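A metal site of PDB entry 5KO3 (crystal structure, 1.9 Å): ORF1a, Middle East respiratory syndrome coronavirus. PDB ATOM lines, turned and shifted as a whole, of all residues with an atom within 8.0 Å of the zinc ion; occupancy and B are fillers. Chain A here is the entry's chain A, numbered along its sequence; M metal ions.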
ATOM      1  N   TRP A 128      32.976 -20.761   2.039  1.00  0.00           N
ATOM      2  CA  TRP A 128      32.516 -19.924   0.944  1.00  0.00           C
ATOM      3  C   TRP A 128      31.495 -20.659   0.087  1.00  0.00           C
ATOM      4  O   TRP A 128      31.689 -21.815  -0.307  1.00  0.00           O
ATOM      5  CB  TRP A 128      33.704 -19.439   0.095  1.00  0.00           C
ATOM      6  CG  TRP A 128      34.323 -20.452  -0.844  1.00  0.00           C
ATOM      7  CD1 TRP A 128      33.935 -20.727  -2.123  1.00  0.00           C
ATOM      8  CD2 TRP A 128      35.462 -21.295  -0.599  1.00  0.00           C
ATOM      9  NE1 TRP A 128      34.742 -21.698  -2.673  1.00  0.00           N
ATOM     10  CE2 TRP A 128      35.700 -22.057  -1.757  1.00  0.00           C
ATOM     11  CE3 TRP A 128      36.303 -21.480   0.513  1.00  0.00           C
ATOM     12  CZ2 TRP A 128      36.726 -22.989  -1.844  1.00  0.00           C
ATOM     13  CZ3 TRP A 128      37.335 -22.404   0.411  1.00  0.00           C
ATOM     14  CH2 TRP A 128      37.538 -23.137  -0.753  1.00  0.00           C
ATOM     15  N   CYS A 129      30.397 -19.959  -0.181  1.00  0.00           N
ATOM     16  CA  CYS A 129      29.332 -20.431  -1.051  1.00  0.00           C
ATOM     17  C   CYS A 129      29.268 -19.520  -2.272  1.00  0.00           C
ATOM     18  O   CYS A 129      29.721 -18.373  -2.214  1.00  0.00           O
ATOM     19  CB  CYS A 129      27.996 -20.452  -0.300  1.00  0.00           C
ATOM     20  SG  CYS A 129      26.518 -20.559  -1.335  1.00  0.00           S
ATOM     21  N   ASN A 130      28.721 -20.020  -3.369  1.00  0.00           N
ATOM     22  CA  ASN A 130      28.581 -19.188  -4.560  1.00  0.00           C
ATOM     23  C   ASN A 130      27.479 -18.161  -4.350  1.00  0.00           C
ATOM     24  O   ASN A 130      27.422 -17.133  -5.026  1.00  0.00           O
ATOM     25  CB  ASN A 130      28.312 -20.043  -5.794  1.00  0.00           C
ATOM     26  CG  ASN A 130      29.172 -19.643  -6.974  1.00  0.00           C
ATOM     27  OD1 ASN A 130      28.792 -18.794  -7.777  1.00  0.00           O
ATOM     28  ND2 ASN A 130      30.354 -20.247  -7.073  1.00  0.00           N
ATOM     29  N   VAL A 131      26.599 -18.448  -3.391  1.00  0.00           N
ATOM     30  CA  VAL A 131      25.584 -17.492  -2.972  1.00  0.00           C
ATOM     31  C   VAL A 131      26.113 -16.607  -1.827  1.00  0.00           C
ATOM     32  O   VAL A 131      26.346 -15.415  -2.014  1.00  0.00           O
ATOM     33  CB  VAL A 131      24.287 -18.194  -2.500  1.00  0.00           C
ATOM     34  CG1 VAL A 131      23.187 -17.181  -2.220  1.00  0.00           C
ATOM     35  CG2 VAL A 131      23.838 -19.213  -3.535  1.00  0.00           C
ATOM     36  N   CYS A 132      26.317 -17.225  -0.678  1.00  0.00           N
ATOM     37  CA  CYS A 132      26.577 -16.524   0.583  1.00  0.00           C
ATOM     38  C   CYS A 132      27.860 -15.697   0.632  1.00  0.00           C
ATOM     39  O   CYS A 132      27.960 -14.776   1.445  1.00  0.00           O
ATOM     40  CB  CYS A 132      26.612 -17.538   1.731  1.00  0.00           C
ATOM     41  SG  CYS A 132      25.057 -18.395   1.977  1.00  0.00           S
ATOM     42  N   GLY A 133      28.831 -16.016  -0.217  1.00  0.00           N
ATOM     43  CA  GLY A 133      30.103 -15.327  -0.177  1.00  0.00           C
ATOM     44  C   GLY A 133      31.127 -16.052   0.688  1.00  0.00           C
ATOM     45  O   GLY A 133      31.125 -17.281   0.752  1.00  0.00           O
ATOM     46  N   VAL A 163      26.340 -29.266   1.530  1.00  0.00           N
ATOM     47  CA  VAL A 163      25.072 -28.586   1.284  1.00  0.00           C
ATOM     48  C   VAL A 163      24.948 -27.402   2.224  1.00  0.00           C
ATOM     49  O   VAL A 163      25.068 -27.546   3.441  1.00  0.00           O
ATOM     50  CB  VAL A 163      23.873 -29.528   1.470  1.00  0.00           C
ATOM     51  CG1 VAL A 163      22.578 -28.824   1.065  1.00  0.00           C
ATOM     52  CG2 VAL A 163      24.067 -30.798   0.668  1.00  0.00           C
ATOM     53  N   CYS A 164      24.709 -26.220   1.657  1.00  0.00           N
ATOM     54  CA  CYS A 164      24.717 -24.991   2.426  1.00  0.00           C
ATOM     55  C   CYS A 164      23.467 -24.815   3.289  1.00  0.00           C
ATOM     56  O   CYS A 164      23.201 -25.606   4.203  1.00  0.00           O
ATOM     57  CB  CYS A 164      24.875 -23.803   1.480  1.00  0.00           C
ATOM     58  SG  CYS A 164      25.257 -22.251   2.285  1.00  0.00           S
ATOM     59  N   GLN A 165      22.703 -23.778   2.986  1.00  0.00           N
ATOM     60  CA  GLN A 165      21.476 -23.458   3.712  1.00  0.00           C
ATOM     61  C   GLN A 165      20.428 -22.946   2.732  1.00  0.00           C
ATOM     62  O   GLN A 165      19.255 -23.304   2.803  1.00  0.00           O
ATOM     63  CB  GLN A 165      21.749 -22.415   4.789  1.00  0.00           C
ATOM     64  CG  GLN A 165      22.273 -21.106   4.216  1.00  0.00           C
ATOM     65  CD  GLN A 165      22.740 -20.142   5.278  1.00  0.00           C
ATOM     66  OE1 GLN A 165      23.093 -20.545   6.382  1.00  0.00           O
ATOM     67  NE2 GLN A 165      22.761 -18.859   4.945  1.00  0.00           N
ATOM     68  N   CYS A 166      20.898 -22.113   1.809  1.00  0.00           N
ATOM     69  CA  CYS A 166      20.060 -21.518   0.774  1.00  0.00           C
ATOM     70  C   CYS A 166      19.688 -22.513  -0.319  1.00  0.00           C
ATOM     71  O   CYS A 166      18.567 -22.511  -0.831  1.00  0.00           O
ATOM     72  CB  CYS A 166      20.762 -20.303   0.165  1.00  0.00           C
ATOM     73  SG  CYS A 166      22.516 -20.592  -0.257  1.00  0.00           S
ATOM     74  N   GLY A 167      20.648 -23.373  -0.669  1.00  0.00           N
ATOM     75  CA  GLY A 167      20.458 -24.341  -1.734  1.00  0.00           C
ATOM     76  C   GLY A 167      21.667 -24.430  -2.639  1.00  0.00           C
ATOM     77  O   GLY A 167      21.742 -25.291  -3.520  1.00  0.00           O
ATOM     78  N   GLY A 168      22.617 -23.527  -2.421  1.00  0.00           N
ATOM     79  CA  GLY A 168      23.858 -23.530  -3.169  1.00  0.00           C
ATOM     80  C   GLY A 168      24.906 -24.401  -2.491  1.00  0.00           C
ATOM     81  O   GLY A 168      24.815 -24.666  -1.295  1.00  0.00           O
ATOM     82  N   GLU A 169      25.882 -24.858  -3.256  1.00  0.00           N
ATOM     83  CA  GLU A 169      26.948 -25.695  -2.712  1.00  0.00           C
ATOM     84  C   GLU A 169      27.964 -24.875  -1.931  1.00  0.00           C
ATOM     85  O   GLU A 169      28.508 -23.894  -2.437  1.00  0.00           O
ATOM     86  CB  GLU A 169      27.645 -26.473  -3.821  1.00  0.00           C
ATOM     87  CG  GLU A 169      28.218 -25.590  -4.918  1.00  0.00           C
ATOM     88  CD  GLU A 169      29.089 -26.373  -5.872  1.00  0.00           C
ATOM     89  OE1 GLU A 169      29.631 -27.420  -5.453  1.00  0.00           O
ATOM     90  OE2 GLU A 169      29.242 -25.938  -7.035  1.00  0.00           O
ATOM     91  N   ARG A 170      28.208 -25.271  -0.689  1.00  0.00           N
ATOM     92  CA  ARG A 170      29.132 -24.555   0.180  1.00  0.00           C
ATOM     93  C   ARG A 170      30.471 -25.289   0.302  1.00  0.00           C
ATOM     94  O   ARG A 170      30.519 -26.525   0.279  1.00  0.00           O
ATOM     95  CB  ARG A 170      28.510 -24.351   1.570  1.00  0.00           C
ATOM     96  CG  ARG A 170      29.308 -23.444   2.486  1.00  0.00           C
ATOM     97  CD  ARG A 170      28.796 -23.558   3.909  1.00  0.00           C
ATOM     98  NE  ARG A 170      28.477 -24.943   4.251  1.00  0.00           N
ATOM     99  CZ  ARG A 170      29.377 -25.878   4.532  1.00  0.00           C
ATOM    100  NH1 ARG A 170      30.668 -25.574   4.525  1.00  0.00           N
ATOM    101  NH2 ARG A 170      28.997 -27.117   4.813  1.00  0.00           N
ATOM    102  N   HIS A 171      31.553 -24.523   0.407  1.00  0.00           N
ATOM    103  CA  HIS A 171      32.890 -25.086   0.514  1.00  0.00           C
ATOM    104  C   HIS A 171      33.590 -24.678   1.808  1.00  0.00           C
ATOM    105  O   HIS A 171      33.401 -23.570   2.317  1.00  0.00           O
ATOM    106  CB  HIS A 171      33.748 -24.667  -0.678  1.00  0.00           C
ATOM    107  CG  HIS A 171      33.361 -25.331  -1.960  1.00  0.00           C
ATOM    108  ND1 HIS A 171      33.772 -24.880  -3.193  1.00  0.00           N
ATOM    109  CD2 HIS A 171      32.599 -26.424  -2.191  1.00  0.00           C
ATOM    110  CE1 HIS A 171      33.277 -25.661  -4.129  1.00  0.00           C
ATOM    111  NE2 HIS A 171      32.561 -26.606  -3.551  1.00  0.00           N
HETATM  112 ZN    ZN M   1      24.843 -20.445   0.723  1.00  0.00          ZN
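SG of Cys 166 lies close to N of Gly 168. The side-chain sulfur of Cys 129 lies close to the backbone NH of Val 131, 2.9 Å away. SG of Cys 132 lies close to NE2 of Gln 165, 3.8 Å away.
The zinc ion is bound by the side-chain sulfur of Cys 132 (2.4 Å), the side-chain sulfur of Cys 164 (2.4 Å), the side-chain sulfur of Cys 166 (2.5 Å) and the side-chain sulfur of Cys 129 (2.7 Å). The zinc ion has four donor atoms within binding distance.
Merely in contact with the zinc ion: Val 131. Of the 15 residues printed, 5 come within 4 Å of the zinc ion.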
